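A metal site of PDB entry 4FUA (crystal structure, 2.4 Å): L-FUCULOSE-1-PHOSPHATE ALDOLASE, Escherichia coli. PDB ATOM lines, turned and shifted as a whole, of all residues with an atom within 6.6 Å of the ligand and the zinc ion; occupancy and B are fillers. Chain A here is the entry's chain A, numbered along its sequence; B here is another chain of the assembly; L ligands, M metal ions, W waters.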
ATOM      1  N   ASN A  23     -21.660 -18.573   6.571  1.00  0.00           N
ATOM      2  CA  ASN A  23     -20.243 -18.389   6.831  1.00  0.00           C
ATOM      3  C   ASN A  23     -19.585 -19.744   6.956  1.00  0.00           C
ATOM      4  O   ASN A  23     -20.213 -20.707   7.391  1.00  0.00           O
ATOM      5  CB  ASN A  23     -20.089 -17.633   8.148  1.00  0.00           C
ATOM      6  CG  ASN A  23     -18.640 -17.249   8.447  1.00  0.00           C
ATOM      7  OD1 ASN A  23     -18.040 -16.441   7.739  1.00  0.00           O
ATOM      8  ND2 ASN A  23     -18.091 -17.811   9.529  1.00  0.00           N
ATOM      9  N   THR A  26     -12.370 -19.844   8.292  1.00  0.00           N
ATOM     10  CA  THR A  26     -11.859 -19.046   9.401  1.00  0.00           C
ATOM     11  C   THR A  26     -12.375 -17.618   9.284  1.00  0.00           C
ATOM     12  O   THR A  26     -11.983 -16.730  10.051  1.00  0.00           O
ATOM     13  CB  THR A  26     -10.289 -19.048   9.437  1.00  0.00           C
ATOM     14  OG1 THR A  26      -9.765 -18.665   8.152  1.00  0.00           O
ATOM     15  CG2 THR A  26      -9.769 -20.431   9.801  1.00  0.00           C
ATOM     16  N   ALA A  27     -13.273 -17.405   8.326  1.00  0.00           N
ATOM     17  CA  ALA A  27     -13.869 -16.106   8.082  1.00  0.00           C
ATOM     18  C   ALA A  27     -14.895 -15.727   9.142  1.00  0.00           C
ATOM     19  O   ALA A  27     -15.419 -16.585   9.856  1.00  0.00           O
ATOM     20  CB  ALA A  27     -14.506 -16.095   6.701  1.00  0.00           C
ATOM     21  N   GLY A  28     -15.178 -14.447   9.249  1.00  0.00           N
ATOM     22  CA  GLY A  28     -16.159 -13.998  10.213  1.00  0.00           C
ATOM     23  C   GLY A  28     -15.683 -13.721  11.623  1.00  0.00           C
ATOM     24  O   GLY A  28     -14.637 -14.186  12.070  1.00  0.00           O
ATOM     25  N   ASN A  29     -16.461 -12.897  12.305  1.00  0.00           N
ATOM     26  CA  ASN A  29     -16.207 -12.505  13.673  1.00  0.00           C
ATOM     27  C   ASN A  29     -17.498 -11.971  14.283  1.00  0.00           C
ATOM     28  O   ASN A  29     -18.400 -11.521  13.591  1.00  0.00           O
ATOM     29  CB  ASN A  29     -15.033 -11.506  13.780  1.00  0.00           C
ATOM     30  CG  ASN A  29     -14.877 -10.600  12.563  1.00  0.00           C
ATOM     31  OD1 ASN A  29     -15.596  -9.628  12.409  1.00  0.00           O
ATOM     32  ND2 ASN A  29     -13.897 -10.904  11.708  1.00  0.00           N
ATOM     33  N   VAL A  30     -17.618 -12.114  15.589  1.00  0.00           N
ATOM     34  CA  VAL A  30     -18.816 -11.666  16.266  1.00  0.00           C
ATOM     35  C   VAL A  30     -18.398 -11.073  17.583  1.00  0.00           C
ATOM     36  O   VAL A  30     -17.431 -11.549  18.188  1.00  0.00           O
ATOM     37  CB  VAL A  30     -19.755 -12.847  16.566  1.00  0.00           C
ATOM     38  CG1 VAL A  30     -20.928 -12.400  17.363  1.00  0.00           C
ATOM     39  CG2 VAL A  30     -20.212 -13.489  15.274  1.00  0.00           C
ATOM     40  N   ILE A  40     -15.339 -10.020  21.952  1.00  0.00           N
ATOM     41  CA  ILE A  40     -15.228 -10.376  20.552  1.00  0.00           C
ATOM     42  C   ILE A  40     -14.455 -11.664  20.354  1.00  0.00           C
ATOM     43  O   ILE A  40     -13.548 -11.990  21.117  1.00  0.00           O
ATOM     44  CB  ILE A  40     -14.523  -9.243  19.753  1.00  0.00           C
ATOM     45  CG1 ILE A  40     -14.686  -9.482  18.238  1.00  0.00           C
ATOM     46  CG2 ILE A  40     -13.052  -9.143  20.140  1.00  0.00           C
ATOM     47  CD1 ILE A  40     -14.337  -8.292  17.388  1.00  0.00           C
ATOM     48  N   THR A  41     -14.809 -12.398  19.307  1.00  0.00           N
ATOM     49  CA  THR A  41     -14.159 -13.649  18.995  1.00  0.00           C
ATOM     50  C   THR A  41     -12.700 -13.396  18.702  1.00  0.00           C
ATOM     51  O   THR A  41     -12.303 -12.273  18.411  1.00  0.00           O
ATOM     52  CB  THR A  41     -14.825 -14.310  17.778  1.00  0.00           C
ATOM     53  OG1 THR A  41     -14.982 -13.354  16.736  1.00  0.00           O
ATOM     54  CG2 THR A  41     -16.189 -14.835  18.146  1.00  0.00           C
ATOM     55  N   PRO A  42     -11.861 -14.410  18.919  1.00  0.00           N
ATOM     56  CA  PRO A  42     -10.436 -14.242  18.651  1.00  0.00           C
ATOM     57  C   PRO A  42     -10.101 -14.544  17.202  1.00  0.00           C
ATOM     58  O   PRO A  42     -10.791 -15.339  16.531  1.00  0.00           O
ATOM     59  CB  PRO A  42      -9.815 -15.252  19.606  1.00  0.00           C
ATOM     60  CG  PRO A  42     -10.782 -16.359  19.581  1.00  0.00           C
ATOM     61  CD  PRO A  42     -12.098 -15.623  19.710  1.00  0.00           C
ATOM     62  N   THR A  43      -9.015 -13.922  16.765  1.00  0.00           N
ATOM     63  CA  THR A  43      -8.529 -14.053  15.400  1.00  0.00           C
ATOM     64  C   THR A  43      -8.026 -15.441  15.027  1.00  0.00           C
ATOM     65  O   THR A  43      -7.157 -16.015  15.694  1.00  0.00           O
ATOM     66  CB  THR A  43      -7.428 -13.006  15.079  1.00  0.00           C
ATOM     67  OG1 THR A  43      -6.969 -13.194  13.736  1.00  0.00           O
ATOM     68  CG2 THR A  43      -6.233 -13.136  16.022  1.00  0.00           C
ATOM     69  N   GLY A  44      -8.626 -15.989  13.972  1.00  0.00           N
ATOM     70  CA  GLY A  44      -8.238 -17.280  13.453  1.00  0.00           C
ATOM     71  C   GLY A  44      -8.403 -18.569  14.234  1.00  0.00           C
ATOM     72  O   GLY A  44      -7.599 -19.479  14.061  1.00  0.00           O
ATOM     73  N   ILE A  45      -9.408 -18.656  15.104  1.00  0.00           N
ATOM     74  CA  ILE A  45      -9.604 -19.899  15.842  1.00  0.00           C
ATOM     75  C   ILE A  45     -10.944 -20.474  15.444  1.00  0.00           C
ATOM     76  O   ILE A  45     -11.974 -19.845  15.660  1.00  0.00           O
ATOM     77  CB  ILE A  45      -9.560 -19.684  17.358  1.00  0.00           C
ATOM     78  CG1 ILE A  45      -8.121 -19.373  17.801  1.00  0.00           C
ATOM     79  CG2 ILE A  45     -10.061 -20.914  18.091  1.00  0.00           C
ATOM     80  CD1 ILE A  45      -7.987 -19.017  19.259  1.00  0.00           C
ATOM     81  N   PRO A  70      -7.415 -10.493  19.776  1.00  0.00           N
ATOM     82  CA  PRO A  70      -8.786 -10.246  19.300  1.00  0.00           C
ATOM     83  C   PRO A  70      -8.865 -10.327  17.774  1.00  0.00           C
ATOM     84  O   PRO A  70      -7.839 -10.358  17.091  1.00  0.00           O
ATOM     85  CB  PRO A  70      -9.078  -8.848  19.834  1.00  0.00           C
ATOM     86  CG  PRO A  70      -7.771  -8.200  19.797  1.00  0.00           C
ATOM     87  CD  PRO A  70      -6.834  -9.262  20.323  1.00  0.00           C
ATOM     88  N   SER A  71     -10.081 -10.405  17.269  1.00  0.00           N
ATOM     89  CA  SER A  71     -10.304 -10.476  15.828  1.00  0.00           C
ATOM     90  C   SER A  71      -9.640  -9.293  15.144  1.00  0.00           C
ATOM     91  O   SER A  71      -9.728  -8.170  15.625  1.00  0.00           O
ATOM     92  CB  SER A  71     -11.801 -10.452  15.523  1.00  0.00           C
ATOM     93  OG  SER A  71     -12.051 -10.150  14.173  1.00  0.00           O
ATOM     94  N   SER A  72      -8.996  -9.557  14.012  1.00  0.00           N
ATOM     95  CA  SER A  72      -8.320  -8.533  13.222  1.00  0.00           C
ATOM     96  C   SER A  72      -9.261  -7.374  12.881  1.00  0.00           C
ATOM     97  O   SER A  72      -8.848  -6.236  12.685  1.00  0.00           O
ATOM     98  CB  SER A  72      -7.735  -9.132  11.935  1.00  0.00           C
ATOM     99  OG  SER A  72      -8.752  -9.592  11.040  1.00  0.00           O
ATOM    100  N   GLU A  73     -10.554  -7.674  12.874  1.00  0.00           N
ATOM    101  CA  GLU A  73     -11.548  -6.678  12.542  1.00  0.00           C
ATOM    102  C   GLU A  73     -12.087  -5.940  13.744  1.00  0.00           C
ATOM    103  O   GLU A  73     -13.000  -5.131  13.592  1.00  0.00           O
ATOM    104  CB  GLU A  73     -12.701  -7.327  11.780  1.00  0.00           C
ATOM    105  CG  GLU A  73     -12.264  -8.127  10.568  1.00  0.00           C
ATOM    106  CD  GLU A  73     -11.707  -7.267   9.435  1.00  0.00           C
ATOM    107  OE1 GLU A  73     -11.512  -6.040   9.589  1.00  0.00           O
ATOM    108  OE2 GLU A  73     -11.446  -7.853   8.359  1.00  0.00           O
ATOM    109  N   PHE A  76     -13.539  -2.304  13.336  1.00  0.00           N
ATOM    110  CA  PHE A  76     -14.816  -2.000  12.710  1.00  0.00           C
ATOM    111  C   PHE A  76     -16.030  -2.463  13.512  1.00  0.00           C
ATOM    112  O   PHE A  76     -17.174  -2.187  13.138  1.00  0.00           O
ATOM    113  CB  PHE A  76     -14.851  -2.372  11.197  1.00  0.00           C
ATOM    114  CG  PHE A  76     -15.108  -3.835  10.883  1.00  0.00           C
ATOM    115  CD1 PHE A  76     -15.960  -4.623  11.629  1.00  0.00           C
ATOM    116  CD2 PHE A  76     -14.546  -4.388   9.722  1.00  0.00           C
ATOM    117  CE1 PHE A  76     -16.268  -5.925  11.239  1.00  0.00           C
ATOM    118  CE2 PHE A  76     -14.842  -5.691   9.320  1.00  0.00           C
ATOM    119  CZ  PHE A  76     -15.707  -6.464  10.075  1.00  0.00           C
ATOM    120  N   HIS A  92     -20.295 -10.468  11.596  1.00  0.00           N
ATOM    121  CA  HIS A  92     -19.585 -10.314  10.348  1.00  0.00           C
ATOM    122  C   HIS A  92     -19.310 -11.670   9.744  1.00  0.00           C
ATOM    123  O   HIS A  92     -18.800 -12.548  10.409  1.00  0.00           O
ATOM    124  CB  HIS A  92     -18.243  -9.615  10.539  1.00  0.00           C
ATOM    125  CG  HIS A  92     -17.381  -9.652   9.315  1.00  0.00           C
ATOM    126  ND1 HIS A  92     -17.763  -9.141   8.086  1.00  0.00           N
ATOM    127  CD2 HIS A  92     -16.152 -10.197   9.128  1.00  0.00           C
ATOM    128  CE1 HIS A  92     -16.777  -9.397   7.215  1.00  0.00           C
ATOM    129  NE2 HIS A  92     -15.780 -10.026   7.804  1.00  0.00           N
ATOM    130  N   ASN A  93     -19.576 -11.805   8.463  1.00  0.00           N
ATOM    131  CA  ASN A  93     -19.316 -13.061   7.794  1.00  0.00           C
ATOM    132  C   ASN A  93     -19.012 -12.852   6.335  1.00  0.00           C
ATOM    133  O   ASN A  93     -19.220 -11.771   5.807  1.00  0.00           O
ATOM    134  CB  ASN A  93     -20.501 -13.991   7.948  1.00  0.00           C
ATOM    135  CG  ASN A  93     -21.753 -13.437   7.358  1.00  0.00           C
ATOM    136  OD1 ASN A  93     -21.760 -12.936   6.224  1.00  0.00           O
ATOM    137  ND2 ASN A  93     -22.833 -13.521   8.106  1.00  0.00           N
ATOM    138  N   HIS A  94     -18.515 -13.900   5.683  1.00  0.00           N
ATOM    139  CA  HIS A  94     -18.238 -13.828   4.240  1.00  0.00           C
ATOM    140  C   HIS A  94     -19.274 -14.694   3.494  1.00  0.00           C
ATOM    141  O   HIS A  94     -18.932 -15.564   2.689  1.00  0.00           O
ATOM    142  CB  HIS A  94     -16.827 -14.311   3.922  1.00  0.00           C
ATOM    143  CG  HIS A  94     -15.735 -13.432   4.463  1.00  0.00           C
ATOM    144  ND1 HIS A  94     -14.416 -13.566   4.122  1.00  0.00           N
ATOM    145  CD2 HIS A  94     -15.782 -12.414   5.357  1.00  0.00           C
ATOM    146  CE1 HIS A  94     -13.703 -12.648   4.815  1.00  0.00           C
ATOM    147  NE2 HIS A  94     -14.489 -11.925   5.574  1.00  0.00           N
ATOM    148  N   PHE A 131      -8.358  -5.391   4.959  1.00  0.00           N
ATOM    149  CA  PHE A 131      -9.030  -5.940   6.137  1.00  0.00           C
ATOM    150  C   PHE A 131      -8.227  -5.575   7.368  1.00  0.00           C
ATOM    151  O   PHE A 131      -7.032  -5.378   7.278  1.00  0.00           O
ATOM    152  CB  PHE A 131      -9.157  -7.471   6.060  1.00  0.00           C
ATOM    153  CG  PHE A 131      -7.872  -8.190   6.229  1.00  0.00           C
ATOM    154  CD1 PHE A 131      -7.399  -8.493   7.505  1.00  0.00           C
ATOM    155  CD2 PHE A 131      -7.099  -8.530   5.124  1.00  0.00           C
ATOM    156  CE1 PHE A 131      -6.164  -9.118   7.662  1.00  0.00           C
ATOM    157  CE2 PHE A 131      -5.864  -9.149   5.273  1.00  0.00           C
ATOM    158  CZ  PHE A 131      -5.391  -9.453   6.548  1.00  0.00           C
ATOM    159  N   GLY A 132      -8.927  -5.441   8.496  1.00  0.00           N
ATOM    160  CA  GLY A 132      -8.287  -5.113   9.767  1.00  0.00           C
ATOM    161  C   GLY A 132      -7.549  -3.782   9.787  1.00  0.00           C
ATOM    162  O   GLY A 132      -6.653  -3.569  10.595  1.00  0.00           O
ATOM    163  N   LEU A 136     -10.760   1.002   6.948  1.00  0.00           N
ATOM    164  CA  LEU A 136     -11.879   0.123   6.695  1.00  0.00           C
ATOM    165  C   LEU A 136     -12.956   0.473   7.708  1.00  0.00           C
ATOM    166  O   LEU A 136     -14.145   0.358   7.433  1.00  0.00           O
ATOM    167  CB  LEU A 136     -11.471  -1.328   6.888  1.00  0.00           C
ATOM    168  CG  LEU A 136     -12.145  -2.442   6.078  1.00  0.00           C
ATOM    169  CD1 LEU A 136     -12.192  -3.639   6.961  1.00  0.00           C
ATOM    170  CD2 LEU A 136     -13.530  -2.079   5.607  1.00  0.00           C
ATOM    171  N   LEU A 152     -19.392  -5.137   2.370  1.00  0.00           N
ATOM    172  CA  LEU A 152     -18.023  -4.616   2.360  1.00  0.00           C
ATOM    173  C   LEU A 152     -17.494  -4.988   0.969  1.00  0.00           C
ATOM    174  O   LEU A 152     -17.456  -6.175   0.624  1.00  0.00           O
ATOM    175  CB  LEU A 152     -17.207  -5.298   3.470  1.00  0.00           C
ATOM    176  CG  LEU A 152     -17.812  -5.228   4.872  1.00  0.00           C
ATOM    177  CD1 LEU A 152     -17.346  -6.372   5.742  1.00  0.00           C
ATOM    178  CD2 LEU A 152     -17.475  -3.929   5.514  1.00  0.00           C
ATOM    179  N   HIS A 155     -15.320  -8.067   0.037  1.00  0.00           N
ATOM    180  CA  HIS A 155     -15.068  -8.668   1.344  1.00  0.00           C
ATOM    181  C   HIS A 155     -16.183  -9.527   1.911  1.00  0.00           C
ATOM    182  O   HIS A 155     -16.021 -10.732   2.040  1.00  0.00           O
ATOM    183  CB  HIS A 155     -14.658  -7.585   2.338  1.00  0.00           C
ATOM    184  CG  HIS A 155     -14.184  -8.111   3.657  1.00  0.00           C
ATOM    185  ND1 HIS A 155     -13.209  -7.501   4.422  1.00  0.00           N
ATOM    186  CD2 HIS A 155     -14.577  -9.199   4.357  1.00  0.00           C
ATOM    187  CE1 HIS A 155     -13.060  -8.225   5.534  1.00  0.00           C
ATOM    188  NE2 HIS A 155     -13.868  -9.265   5.549  1.00  0.00           N
ATOM    189  N   GLY A 156     -17.271  -8.900   2.351  1.00  0.00           N
ATOM    190  CA  GLY A 156     -18.357  -9.674   2.927  1.00  0.00           C
ATOM    191  C   GLY A 156     -19.535  -8.840   3.393  1.00  0.00           C
ATOM    192  O   GLY A 156     -19.934  -7.884   2.737  1.00  0.00           O
ATOM    193  N   TYR B 113      -9.956 -10.709  -1.478  1.00  0.00           N
ATOM    194  CA  TYR B 113      -8.639 -10.676  -0.854  1.00  0.00           C
ATOM    195  C   TYR B 113      -8.140 -12.032  -0.352  1.00  0.00           C
ATOM    196  O   TYR B 113      -6.951 -12.214  -0.106  1.00  0.00           O
ATOM    197  CB  TYR B 113      -8.605  -9.626   0.257  1.00  0.00           C
ATOM    198  CG  TYR B 113      -9.228 -10.056   1.565  1.00  0.00           C
ATOM    199  CD1 TYR B 113      -8.523 -10.866   2.465  1.00  0.00           C
ATOM    200  CD2 TYR B 113     -10.509  -9.664   1.913  1.00  0.00           C
ATOM    201  CE1 TYR B 113      -9.103 -11.273   3.659  1.00  0.00           C
ATOM    202  CE2 TYR B 113     -11.089 -10.071   3.106  1.00  0.00           C
ATOM    203  CZ  TYR B 113     -10.379 -10.880   3.970  1.00  0.00           C
ATOM    204  OH  TYR B 113     -10.923 -11.261   5.171  1.00  0.00           O
HETATM  205  C1  LIG L   1     -12.494 -12.090   8.948  1.00  0.00           C
HETATM  206  C2  LIG L   1     -11.868 -13.130   9.896  1.00  0.00           C
HETATM  207  N1  LIG L   1     -11.792 -10.939   8.786  1.00  0.00           N
HETATM  208  O1  LIG L   1     -12.395 -10.046   7.959  1.00  0.00           O
HETATM  209  O2  LIG L   1     -13.554 -12.278   8.365  1.00  0.00           O
HETATM  210  O3  LIG L   1     -10.841 -12.536  10.664  1.00  0.00           O
HETATM  211  O4  LIG L   1      -9.329 -12.078  12.458  1.00  0.00           O
HETATM  212  O5  LIG L   1     -10.327 -14.440  12.208  1.00  0.00           O
HETATM  213  O6  LIG L   1     -11.797 -12.454  12.972  1.00  0.00           O
HETATM  214  P1  LIG L   1     -10.552 -12.935  12.119  1.00  0.00           P
HETATM  215 ZN    ZN M   1     -13.905 -10.640   7.000  1.00  0.00          ZN
HETATM  216  O   HOH W   1      -9.103 -12.364   7.478  1.00  0.00           O
HETATM  217  O   HOH W   2     -12.971 -13.693  15.003  1.00  0.00           O
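The backbone NH (N) of Gly 28 sits close to an oxygen (O2) of the ligand (2.9 Å). The side-chain hydroxyl (OG) of Ser 71 sits at hydrogen-bond distance from an oxygen (O6) of the ligand, 2.6 Å away. The backbone NH (N) of Gly 44 sits at hydrogen-bond distance from an oxygen (O5) of the ligand. The side-chain hydroxyl (OG1) of Thr 43 sits at hydrogen-bond distance from an oxygen (O4) of the ligand (2.9 Å). An oxygen (O4) of the ligand sits at hydrogen-bond distance from the side-chain hydroxyl of Ser 72. The backbone NH (N) of Ser 72 sits at hydrogen-bond distance from an oxygen (O4) of the ligand, 3.0 Å away. A nitrogen (N1) of the ligand lies within hydrogen-bond range of the side-chain carboxylate (OE2) of Glu 73 (3.1 Å). OH of Tyr 113 of chain B sits close to O1 of the ligand (3.4 Å). ND2 of Asn 29 sits at hydrogen-bond distance from O6 of the ligand (2.9 Å).
Water W2 lies within hydrogen-bond range of O6 of the ligand (2.7 Å), OG1 of Thr 41 (2.7 Å), O of Pro 42 (3.1 Å) and O of Gly 28 (3.4 Å). Water W1 lies within hydrogen-bond range of OH of Tyr 113 of chain B (3.1 Å) and N1 of the ligand (3.3 Å).
Thr 26 touches the ligand (O to O5, 3.6 Å). C of Ala 27 touches O2 of the ligand, 3.8 Å away. Hydrophobic or aromatic side chains that line the ligand: His 92, His 94 and His 155. 13 residues have an atom within 4 Å of the ligand: Thr 26, Ala 27, Gly 28, Asn 29, Thr 43, Gly 44, Ser 71, Ser 72, Glu 73, His 92, His 94, His 155 and Tyr 113 of chain B.
Glu 73 touches the zinc ion (OE2 to ZN, 3.96 Å). Tyr 113 of chain B touches the zinc ion. Of the 27 residues printed, 5 come within 4 Å of the zinc ion. The nearest printed residue that does not touch the zinc ion is Gly 28 (4.6 Å).
O1 of the ligand is bound to the zinc ion (1.9 Å). NE2 of His 155 binds the zinc ion. A ring nitrogen (NE2) of His 94 binds the zinc ion, 2.0 Å away. The zinc ion is bound by a ring nitrogen (NE2) of His 92, 2.1 Å away. An oxygen (O2) of the ligand is bound to the zinc ion (2.2 Å).
The backbone carbonyl oxygen of Ala 27 is in hydrogen-bond range of the side-chain amide nitrogen of Asn 23 (3.0 Å). The backbone NH (N) of Ser 71 lies within hydrogen-bond range of the backbone carbonyl oxygen (O) of Thr 41 (3.1 Å). OE1 of Glu 73 is in hydrogen-bond range of N of Gly 132 (2.9 Å). The side-chain amide nitrogen (ND2) of Asn 29 is in hydrogen-bond range of the side-chain hydroxyl (OG) of Ser 71 (3.2 Å). O of Asn 29 sits at hydrogen-bond distance from N of His 92 (2.9 Å). N of His 94 lies within hydrogen-bond range of OD1 of Asn 23. N of Glu 73 sits close to OG of Ser 71.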
